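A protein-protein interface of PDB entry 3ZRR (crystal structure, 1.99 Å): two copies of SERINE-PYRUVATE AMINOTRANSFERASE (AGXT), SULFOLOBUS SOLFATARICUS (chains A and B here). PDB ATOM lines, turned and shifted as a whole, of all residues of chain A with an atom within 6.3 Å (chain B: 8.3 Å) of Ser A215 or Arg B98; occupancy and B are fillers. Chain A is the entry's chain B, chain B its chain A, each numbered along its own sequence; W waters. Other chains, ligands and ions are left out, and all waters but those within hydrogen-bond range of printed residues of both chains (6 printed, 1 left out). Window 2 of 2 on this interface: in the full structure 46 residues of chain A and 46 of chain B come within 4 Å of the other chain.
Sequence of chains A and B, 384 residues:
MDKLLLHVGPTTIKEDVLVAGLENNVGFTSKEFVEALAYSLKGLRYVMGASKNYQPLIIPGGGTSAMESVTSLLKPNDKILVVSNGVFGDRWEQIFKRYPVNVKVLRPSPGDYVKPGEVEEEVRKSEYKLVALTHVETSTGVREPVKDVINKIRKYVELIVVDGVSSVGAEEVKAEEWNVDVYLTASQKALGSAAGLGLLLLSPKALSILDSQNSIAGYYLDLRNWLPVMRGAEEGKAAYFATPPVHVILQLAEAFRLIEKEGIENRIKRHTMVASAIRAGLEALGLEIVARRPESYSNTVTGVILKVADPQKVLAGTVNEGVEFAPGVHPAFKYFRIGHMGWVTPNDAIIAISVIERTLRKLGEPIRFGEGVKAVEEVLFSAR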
ATOM      1  N   THR A  71     -14.685 -10.531  -6.742  1.00  0.00           N
ATOM      2  CA  THR A  71     -14.370 -11.972  -6.913  1.00  0.00           C
ATOM      3  C   THR A  71     -15.514 -12.904  -6.418  1.00  0.00           C
ATOM      4  O   THR A  71     -15.551 -14.088  -6.779  1.00  0.00           O
ATOM      5  CB  THR A  71     -13.087 -12.385  -6.179  1.00  0.00           C
ATOM      6  OG1 THR A  71     -13.229 -12.064  -4.783  1.00  0.00           O
ATOM      7  CG2 THR A  71     -11.852 -11.676  -6.781  1.00  0.00           C
ATOM      8  N   SER A  72     -16.435 -12.368  -5.610  1.00  0.00           N
ATOM      9  CA  SER A  72     -17.607 -13.108  -5.145  1.00  0.00           C
ATOM     10  C   SER A  72     -18.510 -13.493  -6.315  1.00  0.00           C
ATOM     11  O   SER A  72     -19.443 -14.311  -6.161  1.00  0.00           O
ATOM     12  CB  SER A  72     -18.461 -12.250  -4.161  1.00  0.00           C
ATOM     13  OG  SER A  72     -17.761 -11.924  -2.967  1.00  0.00           O
ATOM     14  N   LEU A  73     -18.272 -12.858  -7.464  1.00  0.00           N
ATOM     15  CA  LEU A  73     -19.133 -13.041  -8.640  1.00  0.00           C
ATOM     16  C   LEU A  73     -18.432 -13.846  -9.726  1.00  0.00           C
ATOM     17  O   LEU A  73     -18.954 -14.011 -10.834  1.00  0.00           O
ATOM     18  CB  LEU A  73     -19.577 -11.680  -9.182  1.00  0.00           C
ATOM     19  CG  LEU A  73     -20.447 -10.833  -8.238  1.00  0.00           C
ATOM     20  CD1 LEU A  73     -20.761  -9.514  -8.866  1.00  0.00           C
ATOM     21  CD2 LEU A  73     -21.736 -11.527  -7.885  1.00  0.00           C
ATOM     22  N   LEU A  74     -17.245 -14.352  -9.404  1.00  0.00           N
ATOM     23  CA  LEU A  74     -16.394 -14.988 -10.410  1.00  0.00           C
ATOM     24  C   LEU A  74     -16.153 -16.483 -10.151  1.00  0.00           C
ATOM     25  O   LEU A  74     -16.320 -16.968  -9.017  1.00  0.00           O
ATOM     26  CB  LEU A  74     -15.065 -14.229 -10.526  1.00  0.00           C
ATOM     27  CG  LEU A  74     -15.238 -12.754 -10.918  1.00  0.00           C
ATOM     28  CD1 LEU A  74     -13.916 -12.019 -10.783  1.00  0.00           C
ATOM     29  CD2 LEU A  74     -15.829 -12.636 -12.348  1.00  0.00           C
ATOM     30  N   LYS A  75     -15.791 -17.198 -11.218  1.00  0.00           N
ATOM     31  CA  LYS A  75     -15.467 -18.632 -11.163  1.00  0.00           C
ATOM     32  C   LYS A  75     -14.105 -18.888 -11.779  1.00  0.00           C
ATOM     33  O   LYS A  75     -13.634 -18.059 -12.551  1.00  0.00           O
ATOM     34  CB  LYS A  75     -16.538 -19.430 -11.895  1.00  0.00           C
ATOM     35  CG  LYS A  75     -17.734 -19.648 -11.026  1.00  0.00           C
ATOM     36  CD  LYS A  75     -18.865 -20.309 -11.745  1.00  0.00           C
ATOM     37  CE  LYS A  75     -19.851 -20.821 -10.697  1.00  0.00           C
ATOM     38  NZ  LYS A  75     -21.172 -21.143 -11.277  1.00  0.00           N
ATOM     39  N   PRO A  76     -13.453 -20.035 -11.464  1.00  0.00           N
ATOM     40  CA  PRO A  76     -12.112 -20.178 -12.028  1.00  0.00           C
ATOM     41  C   PRO A  76     -12.129 -20.058 -13.572  1.00  0.00           C
ATOM     42  O   PRO A  76     -13.099 -20.494 -14.219  1.00  0.00           O
ATOM     43  CB  PRO A  76     -11.697 -21.597 -11.578  1.00  0.00           C
ATOM     44  CG  PRO A  76     -12.471 -21.817 -10.299  1.00  0.00           C
ATOM     45  CD  PRO A  76     -13.819 -21.208 -10.632  1.00  0.00           C
ATOM     46  N   ILE A 209     -26.284 -14.412  -8.843  1.00  0.00           N
ATOM     47  CA  ILE A 209     -25.014 -15.144  -8.771  1.00  0.00           C
ATOM     48  C   ILE A 209     -24.680 -15.466  -7.307  1.00  0.00           C
ATOM     49  O   ILE A 209     -24.380 -16.619  -6.982  1.00  0.00           O
ATOM     50  CB  ILE A 209     -23.879 -14.372  -9.443  1.00  0.00           C
ATOM     51  CG1 ILE A 209     -24.151 -14.284 -10.941  1.00  0.00           C
ATOM     52  CG2 ILE A 209     -22.520 -15.015  -9.131  1.00  0.00           C
ATOM     53  CD1 ILE A 209     -23.107 -13.525 -11.715  1.00  0.00           C
ATOM     54  N   GLN A 213     -24.840 -19.516  -6.868  1.00  0.00           N
ATOM     55  CA  GLN A 213     -23.577 -20.073  -7.368  1.00  0.00           C
ATOM     56  C   GLN A 213     -22.449 -20.004  -6.335  1.00  0.00           C
ATOM     57  O   GLN A 213     -22.511 -19.228  -5.393  1.00  0.00           O
ATOM     58  CB  GLN A 213     -23.138 -19.352  -8.652  1.00  0.00           C
ATOM     59  CG  GLN A 213     -24.214 -19.239  -9.738  1.00  0.00           C
ATOM     60  CD  GLN A 213     -23.691 -18.696 -11.066  1.00  0.00           C
ATOM     61  OE1 GLN A 213     -22.539 -18.925 -11.436  1.00  0.00           O
ATOM     62  NE2 GLN A 213     -24.550 -17.993 -11.798  1.00  0.00           N
ATOM     63  N   ASN A 214     -21.422 -20.835  -6.528  1.00  0.00           N
ATOM     64  CA  ASN A 214     -20.165 -20.777  -5.758  1.00  0.00           C
ATOM     65  C   ASN A 214     -19.244 -19.699  -6.354  1.00  0.00           C
ATOM     66  O   ASN A 214     -19.552 -19.162  -7.421  1.00  0.00           O
ATOM     67  CB  ASN A 214     -19.427 -22.120  -5.843  1.00  0.00           C
ATOM     68  CG  ASN A 214     -20.174 -23.262  -5.159  1.00  0.00           C
ATOM     69  OD1 ASN A 214     -19.919 -24.436  -5.449  1.00  0.00           O
ATOM     70  ND2 ASN A 214     -21.099 -22.928  -4.260  1.00  0.00           N
ATOM     71  N   SER A 215     -18.099 -19.417  -5.724  1.00  0.00           N
ATOM     72  CA  SER A 215     -17.201 -18.392  -6.262  1.00  0.00           C
ATOM     73  C   SER A 215     -15.798 -18.650  -5.816  1.00  0.00           C
ATOM     74  O   SER A 215     -15.558 -19.532  -5.005  1.00  0.00           O
ATOM     75  CB  SER A 215     -17.635 -16.976  -5.816  1.00  0.00           C
ATOM     76  OG  SER A 215     -17.222 -16.717  -4.481  1.00  0.00           O
ATOM     77  N   ILE A 216     -14.873 -17.850  -6.325  1.00  0.00           N
ATOM     78  CA  ILE A 216     -13.454 -17.962  -5.961  1.00  0.00           C
ATOM     79  C   ILE A 216     -13.064 -17.024  -4.790  1.00  0.00           C
ATOM     80  O   ILE A 216     -11.873 -16.895  -4.445  1.00  0.00           O
ATOM     81  CB  ILE A 216     -12.574 -17.664  -7.184  1.00  0.00           C
ATOM     82  CG1 ILE A 216     -12.852 -16.250  -7.701  1.00  0.00           C
ATOM     83  CG2 ILE A 216     -12.846 -18.722  -8.287  1.00  0.00           C
ATOM     84  CD1 ILE A 216     -12.028 -15.854  -8.912  1.00  0.00           C
ATOM     85  N   ALA A 217     -14.069 -16.385  -4.183  1.00  0.00           N
ATOM     86  CA  ALA A 217     -13.827 -15.427  -3.078  1.00  0.00           C
ATOM     87  C   ALA A 217     -13.183 -16.112  -1.882  1.00  0.00           C
ATOM     88  O   ALA A 217     -13.327 -17.330  -1.704  1.00  0.00           O
ATOM     89  CB  ALA A 217     -15.148 -14.754  -2.650  1.00  0.00           C
ATOM     90  N   GLY A 218     -12.457 -15.337  -1.083  1.00  0.00           N
ATOM     91  CA  GLY A 218     -11.973 -15.808   0.222  1.00  0.00           C
ATOM     92  C   GLY A 218     -13.129 -15.855   1.211  1.00  0.00           C
ATOM     93  O   GLY A 218     -14.287 -16.067   0.834  1.00  0.00           O
ATOM     94  N   TYR A 219     -12.839 -15.610   2.478  1.00  0.00           N
ATOM     95  CA  TYR A 219     -13.887 -15.679   3.499  1.00  0.00           C
ATOM     96  C   TYR A 219     -14.466 -14.288   3.838  1.00  0.00           C
ATOM     97  O   TYR A 219     -15.676 -14.025   3.630  1.00  0.00           O
ATOM     98  CB  TYR A 219     -13.334 -16.405   4.724  1.00  0.00           C
ATOM     99  CG  TYR A 219     -14.346 -16.709   5.812  1.00  0.00           C
ATOM    100  CD1 TYR A 219     -15.240 -17.760   5.681  1.00  0.00           C
ATOM    101  CD2 TYR A 219     -14.381 -15.947   6.978  1.00  0.00           C
ATOM    102  CE1 TYR A 219     -16.157 -18.034   6.679  1.00  0.00           C
ATOM    103  CE2 TYR A 219     -15.283 -16.219   7.981  1.00  0.00           C
ATOM    104  CZ  TYR A 219     -16.166 -17.252   7.822  1.00  0.00           C
ATOM    105  OH  TYR A 219     -17.050 -17.536   8.825  1.00  0.00           O
ATOM    106  N   ASP A 222     -16.204 -12.373   0.844  1.00  0.00           N
ATOM    107  CA  ASP A 222     -17.273 -13.016   0.119  1.00  0.00           C
ATOM    108  C   ASP A 222     -18.553 -12.309   0.510  1.00  0.00           C
ATOM    109  O   ASP A 222     -19.015 -12.436   1.639  1.00  0.00           O
ATOM    110  CB  ASP A 222     -17.348 -14.509   0.477  1.00  0.00           C
ATOM    111  CG  ASP A 222     -18.390 -15.253  -0.329  1.00  0.00           C
ATOM    112  OD1 ASP A 222     -19.200 -14.570  -0.982  1.00  0.00           O
ATOM    113  OD2 ASP A 222     -18.400 -16.507  -0.285  1.00  0.00           O
ATOM    114  N   ARG A 224     -21.443 -12.971  -0.003  1.00  0.00           N
ATOM    115  CA  ARG A 224     -22.436 -13.901   0.572  1.00  0.00           C
ATOM    116  C   ARG A 224     -22.466 -13.848   2.082  1.00  0.00           C
ATOM    117  O   ARG A 224     -23.540 -13.914   2.671  1.00  0.00           O
ATOM    118  CB  ARG A 224     -22.218 -15.345   0.117  1.00  0.00           C
ATOM    119  CG  ARG A 224     -22.504 -15.563  -1.385  1.00  0.00           C
ATOM    120  CD  ARG A 224     -21.843 -16.870  -1.883  1.00  0.00           C
ATOM    121  NE  ARG A 224     -21.952 -16.959  -3.339  1.00  0.00           N
ATOM    122  CZ  ARG A 224     -21.144 -16.344  -4.197  1.00  0.00           C
ATOM    123  NH1 ARG A 224     -20.132 -15.597  -3.756  1.00  0.00           N
ATOM    124  NH2 ARG A 224     -21.342 -16.477  -5.507  1.00  0.00           N
ATOM    125  N   ASN A 225     -21.299 -13.702   2.711  1.00  0.00           N
ATOM    126  CA  ASN A 225     -21.233 -13.712   4.165  1.00  0.00           C
ATOM    127  C   ASN A 225     -21.805 -12.436   4.793  1.00  0.00           C
ATOM    128  O   ASN A 225     -22.296 -12.456   5.939  1.00  0.00           O
ATOM    129  CB  ASN A 225     -19.796 -13.983   4.625  1.00  0.00           C
ATOM    130  CG  ASN A 225     -19.362 -15.413   4.346  1.00  0.00           C
ATOM    131  OD1 ASN A 225     -20.174 -16.315   4.403  1.00  0.00           O
ATOM    132  ND2 ASN A 225     -18.080 -15.627   4.050  1.00  0.00           N
ATOM    133  N   GLU B  68      -7.930 -14.501   8.863  1.00  0.00           N
ATOM    134  CA  GLU B  68      -7.753 -14.865   7.460  1.00  0.00           C
ATOM    135  C   GLU B  68      -6.368 -14.445   6.922  1.00  0.00           C
ATOM    136  O   GLU B  68      -5.767 -15.147   6.102  1.00  0.00           O
ATOM    137  CB  GLU B  68      -8.886 -14.327   6.601  1.00  0.00           C
ATOM    138  CG  GLU B  68      -8.811 -14.718   5.105  1.00  0.00           C
ATOM    139  CD  GLU B  68     -10.150 -14.516   4.400  1.00  0.00           C
ATOM    140  OE1 GLU B  68     -11.113 -14.008   5.048  1.00  0.00           O
ATOM    141  OE2 GLU B  68     -10.242 -14.848   3.208  1.00  0.00           O
ATOM    142  N   THR B  71      -3.328 -16.826   6.208  1.00  0.00           N
ATOM    143  CA  THR B  71      -3.078 -17.450   4.889  1.00  0.00           C
ATOM    144  C   THR B  71      -1.855 -16.826   4.158  1.00  0.00           C
ATOM    145  O   THR B  71      -1.317 -17.428   3.218  1.00  0.00           O
ATOM    146  CB  THR B  71      -4.297 -17.330   3.940  1.00  0.00           C
ATOM    147  OG1 THR B  71      -4.613 -15.938   3.753  1.00  0.00           O
ATOM    148  CG2 THR B  71      -5.514 -18.097   4.480  1.00  0.00           C
ATOM    149  N   TRP B  92     -11.706 -20.864  12.332  1.00  0.00           N
ATOM    150  CA  TRP B  92     -10.470 -21.160  11.600  1.00  0.00           C
ATOM    151  C   TRP B  92     -10.773 -22.127  10.437  1.00  0.00           C
ATOM    152  O   TRP B  92     -10.342 -21.905   9.307  1.00  0.00           O
ATOM    153  CB  TRP B  92      -9.406 -21.801  12.482  1.00  0.00           C
ATOM    154  CG  TRP B  92      -8.662 -20.906  13.418  1.00  0.00           C
ATOM    155  CD1 TRP B  92      -8.693 -20.956  14.788  1.00  0.00           C
ATOM    156  CD2 TRP B  92      -7.731 -19.875  13.073  1.00  0.00           C
ATOM    157  NE1 TRP B  92      -7.841 -20.008  15.313  1.00  0.00           N
ATOM    158  CE2 TRP B  92      -7.250 -19.326  14.277  1.00  0.00           C
ATOM    159  CE3 TRP B  92      -7.278 -19.338  11.857  1.00  0.00           C
ATOM    160  CZ2 TRP B  92      -6.318 -18.279  14.304  1.00  0.00           C
ATOM    161  CZ3 TRP B  92      -6.357 -18.285  11.889  1.00  0.00           C
ATOM    162  CH2 TRP B  92      -5.894 -17.771  13.107  1.00  0.00           C
ATOM    163  N   GLU B  93     -11.511 -23.193  10.735  1.00  0.00           N
ATOM    164  CA  GLU B  93     -11.858 -24.192   9.724  1.00  0.00           C
ATOM    165  C   GLU B  93     -12.722 -23.609   8.597  1.00  0.00           C
ATOM    166  O   GLU B  93     -12.536 -23.950   7.431  1.00  0.00           O
ATOM    167  CB  GLU B  93     -12.548 -25.410  10.374  1.00  0.00           C
ATOM    168  CG  GLU B  93     -13.073 -26.437   9.378  1.00  0.00           C
ATOM    169  CD  GLU B  93     -13.720 -27.638  10.045  1.00  0.00           C
ATOM    170  OE1 GLU B  93     -14.501 -27.447  11.013  1.00  0.00           O
ATOM    171  OE2 GLU B  93     -13.437 -28.776   9.591  1.00  0.00           O
ATOM    172  N   GLN B  94     -13.675 -22.749   8.949  1.00  0.00           N
ATOM    173  CA  GLN B  94     -14.535 -22.104   7.963  1.00  0.00           C
ATOM    174  C   GLN B  94     -13.699 -21.199   7.034  1.00  0.00           C
ATOM    175  O   GLN B  94     -13.908 -21.182   5.807  1.00  0.00           O
ATOM    176  CB  GLN B  94     -15.645 -21.282   8.660  1.00  0.00           C
ATOM    177  CG  GLN B  94     -16.622 -22.115   9.473  1.00  0.00           C
ATOM    178  CD  GLN B  94     -17.385 -23.094   8.585  1.00  0.00           C
ATOM    179  OE1 GLN B  94     -17.239 -24.318   8.700  1.00  0.00           O
ATOM    180  NE2 GLN B  94     -18.171 -22.554   7.662  1.00  0.00           N
ATOM    181  N   ILE B  95     -12.749 -20.465   7.616  1.00  0.00           N
ATOM    182  CA  ILE B  95     -11.861 -19.625   6.824  1.00  0.00           C
ATOM    183  C   ILE B  95     -11.000 -20.515   5.892  1.00  0.00           C
ATOM    184  O   ILE B  95     -10.938 -20.278   4.667  1.00  0.00           O
ATOM    185  CB  ILE B  95     -10.937 -18.757   7.713  1.00  0.00           C
ATOM    186  CG1 ILE B  95     -11.760 -17.701   8.478  1.00  0.00           C
ATOM    187  CG2 ILE B  95      -9.798 -18.107   6.867  1.00  0.00           C
ATOM    188  CD1 ILE B  95     -10.989 -17.053   9.631  1.00  0.00           C
ATOM    189  N   PHE B  96     -10.367 -21.544   6.454  1.00  0.00           N
ATOM    190  CA  PHE B  96      -9.460 -22.370   5.651  1.00  0.00           C
ATOM    191  C   PHE B  96     -10.135 -23.180   4.539  1.00  0.00           C
ATOM    192  O   PHE B  96      -9.465 -23.545   3.584  1.00  0.00           O
ATOM    193  CB  PHE B  96      -8.574 -23.249   6.522  1.00  0.00           C
ATOM    194  CG  PHE B  96      -7.619 -22.481   7.374  1.00  0.00           C
ATOM    195  CD1 PHE B  96      -6.868 -21.431   6.839  1.00  0.00           C
ATOM    196  CD2 PHE B  96      -7.461 -22.804   8.724  1.00  0.00           C
ATOM    197  CE1 PHE B  96      -5.965 -20.722   7.640  1.00  0.00           C
ATOM    198  CE2 PHE B  96      -6.566 -22.095   9.534  1.00  0.00           C
ATOM    199  CZ  PHE B  96      -5.819 -21.050   8.987  1.00  0.00           C
ATOM    200  N   LYS B  97     -11.442 -23.424   4.628  1.00  0.00           N
ATOM    201  CA  LYS B  97     -12.160 -24.060   3.519  1.00  0.00           C
ATOM    202  C   LYS B  97     -12.128 -23.227   2.237  1.00  0.00           C
ATOM    203  O   LYS B  97     -12.388 -23.757   1.152  1.00  0.00           O
ATOM    204  CB  LYS B  97     -13.629 -24.275   3.849  1.00  0.00           C
ATOM    205  CG  LYS B  97     -13.977 -25.466   4.688  1.00  0.00           C
ATOM    206  CD  LYS B  97     -15.524 -25.481   4.759  1.00  0.00           C
ATOM    207  CE  LYS B  97     -16.078 -26.159   6.007  1.00  0.00           C
ATOM    208  NZ  LYS B  97     -15.745 -27.612   6.017  1.00  0.00           N
ATOM    209  N   ARG B  98     -11.847 -21.932   2.352  1.00  0.00           N
ATOM    210  CA  ARG B  98     -11.778 -21.077   1.165  1.00  0.00           C
ATOM    211  C   ARG B  98     -10.397 -21.140   0.498  1.00  0.00           C
ATOM    212  O   ARG B  98     -10.176 -20.454  -0.493  1.00  0.00           O
ATOM    213  CB  ARG B  98     -12.112 -19.635   1.539  1.00  0.00           C
ATOM    214  CG  ARG B  98     -13.510 -19.426   2.150  1.00  0.00           C
ATOM    215  CD  ARG B  98     -14.617 -20.076   1.335  1.00  0.00           C
ATOM    216  NE  ARG B  98     -14.760 -19.430   0.031  1.00  0.00           N
ATOM    217  CZ  ARG B  98     -15.567 -19.845  -0.945  1.00  0.00           C
ATOM    218  NH1 ARG B  98     -16.337 -20.912  -0.780  1.00  0.00           N
ATOM    219  NH2 ARG B  98     -15.601 -19.196  -2.103  1.00  0.00           N
ATOM    220  N   TYR B  99      -9.485 -21.942   1.061  1.00  0.00           N
ATOM    221  CA  TYR B  99      -8.070 -22.004   0.642  1.00  0.00           C
ATOM    222  C   TYR B  99      -7.603 -23.441   0.372  1.00  0.00           C
ATOM    223  O   TYR B  99      -8.107 -24.387   0.993  1.00  0.00           O
ATOM    224  CB  TYR B  99      -7.156 -21.353   1.690  1.00  0.00           C
ATOM    225  CG  TYR B  99      -7.402 -19.863   1.789  1.00  0.00           C
ATOM    226  CD1 TYR B  99      -8.450 -19.352   2.610  1.00  0.00           C
ATOM    227  CD2 TYR B  99      -6.683 -18.968   0.990  1.00  0.00           C
ATOM    228  CE1 TYR B  99      -8.731 -17.996   2.655  1.00  0.00           C
ATOM    229  CE2 TYR B  99      -6.959 -17.593   1.028  1.00  0.00           C
ATOM    230  CZ  TYR B  99      -7.971 -17.114   1.867  1.00  0.00           C
ATOM    231  OH  TYR B  99      -8.235 -15.764   1.915  1.00  0.00           O
ATOM    232  N   PRO B 100      -6.625 -23.607  -0.547  1.00  0.00           N
ATOM    233  CA  PRO B 100      -6.131 -24.949  -0.904  1.00  0.00           C
ATOM    234  C   PRO B 100      -5.179 -25.485   0.153  1.00  0.00           C
ATOM    235  O   PRO B 100      -3.962 -25.566  -0.063  1.00  0.00           O
ATOM    236  CB  PRO B 100      -5.429 -24.724  -2.264  1.00  0.00           C
ATOM    237  CG  PRO B 100      -4.951 -23.292  -2.191  1.00  0.00           C
ATOM    238  CD  PRO B 100      -6.001 -22.550  -1.362  1.00  0.00           C
ATOM    239  N   VAL B 101      -5.744 -25.825   1.308  1.00  0.00           N
ATOM    240  CA  VAL B 101      -4.962 -26.320   2.432  1.00  0.00           C
ATOM    241  C   VAL B 101      -5.660 -27.536   3.039  1.00  0.00           C
ATOM    242  O   VAL B 101      -6.843 -27.791   2.762  1.00  0.00           O
ATOM    243  CB  VAL B 101      -4.737 -25.227   3.525  1.00  0.00           C
ATOM    244  CG1 VAL B 101      -3.884 -24.085   2.995  1.00  0.00           C
ATOM    245  CG2 VAL B 101      -6.091 -24.717   4.061  1.00  0.00           C
ATOM    246  N   VAL B 103      -6.873 -29.340   6.426  1.00  0.00           N
ATOM    247  CA  VAL B 103      -7.227 -29.014   7.808  1.00  0.00           C
ATOM    248  C   VAL B 103      -7.677 -30.218   8.643  1.00  0.00           C
ATOM    249  O   VAL B 103      -8.580 -30.935   8.252  1.00  0.00           O
ATOM    250  CB  VAL B 103      -8.322 -27.923   7.820  1.00  0.00           C
ATOM    251  CG1 VAL B 103      -8.849 -27.694   9.225  1.00  0.00           C
ATOM    252  CG2 VAL B 103      -7.746 -26.622   7.266  1.00  0.00           C
ATOM    253  N   ILE B 216      -0.707 -18.155  -0.501  1.00  0.00           N
ATOM    254  CA  ILE B 216      -2.032 -18.347  -1.095  1.00  0.00           C
ATOM    255  C   ILE B 216      -3.017 -17.199  -0.755  1.00  0.00           C
ATOM    256  O   ILE B 216      -4.217 -17.260  -1.095  1.00  0.00           O
ATOM    257  CB  ILE B 216      -2.619 -19.697  -0.679  1.00  0.00           C
ATOM    258  CG1 ILE B 216      -2.737 -19.755   0.851  1.00  0.00           C
ATOM    259  CG2 ILE B 216      -1.707 -20.848  -1.191  1.00  0.00           C
ATOM    260  CD1 ILE B 216      -3.327 -21.047   1.385  1.00  0.00           C
HETATM  261  O   HOH W   1     -18.260 -21.125  -3.084  1.00  0.00           O
HETATM  262  O   HOH W   2     -18.907 -19.543   8.145  1.00  0.00           O
HETATM  263  O   HOH W   3     -13.802 -21.688  -3.132  1.00  0.00           O
HETATM  264  O   HOH W   4     -18.460 -17.992  -2.613  1.00  0.00           O
HETATM  265  O   HOH W   5     -16.844 -17.492   1.608  1.00  0.00           O
HETATM  266  O   HOH W   6     -11.723 -12.657   1.453  1.00  0.00           O
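OE2 of Glu B68 is in hydrogen-bond range of N of Tyr A219.
NH2 of Arg B98 sits at hydrogen-bond distance from O of Ser A215, at 2.9 Å.
The backbone carbonyl oxygen of Ala A217 sits at hydrogen-bond distance from the guanidinium group of Arg B98 (3.0 Å).
The guanidinium group (NE) of Arg B98 sits at hydrogen-bond distance from the backbone carbonyl oxygen (O) of Gly A218, 3.5 Å away.
O of Glu B68 sits at hydrogen-bond distance from OG1 of Thr B71, 2.7 Å away.
The side-chain carboxylate of Glu B68 sits at hydrogen-bond distance from the side-chain hydroxyl of Tyr B99, at 2.6 Å.
The backbone NH of Ala A217 sits at hydrogen-bond distance from the side-chain hydroxyl of Ser A215, 3.2 Å away.
The side-chain hydroxyl (OG) of Ser A215 is in hydrogen-bond range of the guanidinium group (NH1) of Arg A224.
ND2 of Asn A225 is in hydrogen-bond range of O of Tyr A219 (2.9 Å).
Gly A218 touches Glu B68.
Tyr A219 touches Gln B94.
Tyr A219 touches Ile B95.
Arg B98 touches Tyr A219 (CG to N, 3.9 Å).
Of the printed residues of chain A, Arg B98 touches Ser A215 (2.9 Å), Ala A217 (3.0 Å), Gly A218 (3.5 Å) and Tyr A219 (3.9 Å).
Ala A217 touches one residue of chain B.
Of the printed residues of chain B, Gly A218 touches Glu B68 and Arg B98.
Of the printed residues of chain B, Tyr A219 touches Glu B68, Gln B94, Ile B95 and Arg B98.
Lys A75 touches none of the printed residues of chain B.
The nearest printed residue of chain A that does not touch Arg B98 is Asp A222 (4.3 Å).
Along chain A the printed residues that touch a printed residue of chain B span positions 215 to 219.
Of the 14 printed residues of chain B, 4 touch a printed residue of chain A.
Printed residues of chain B that touch a printed residue of chain A: Glu B68, Gln B94, Ile B95 and Arg B98.
Among the printed residues, 8 pairs touch across the chains.
Positions printed for both chains: 71 and 216.
Water W4 lies within hydrogen-bond range of OG of Ser A215 (2.6 Å), OD2 of Asp A222 (2.8 Å), NH1 of Arg A224 (3.1 Å) and NH2 of Arg B98 (3.1 Å).
Water W5 lies within hydrogen-bond range of OD2 of Asp A222 (2.6 Å), O of Gly A218 (3.0 Å), NE of Arg B98 (3.3 Å) and ND2 of Asn A225 (3.3 Å).
Water W2 bridges the side-chain hydroxyl (OH) of Tyr A219 and the side-chain amide nitrogen (NE2) of Gln B94.
Water W1 lies within hydrogen-bond range of the guanidinium group (NH1) of Arg B98 and the backbone NH (N) of Ser A215.
Water W6 lies within hydrogen-bond range of the side-chain carboxylate of Glu B68 (3.2 Å) and the backbone NH of Tyr A219 (3.3 Å).
Water W3 lies within hydrogen-bond range of the guanidinium group of Arg B98 and the backbone carbonyl oxygen of Ser A215.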
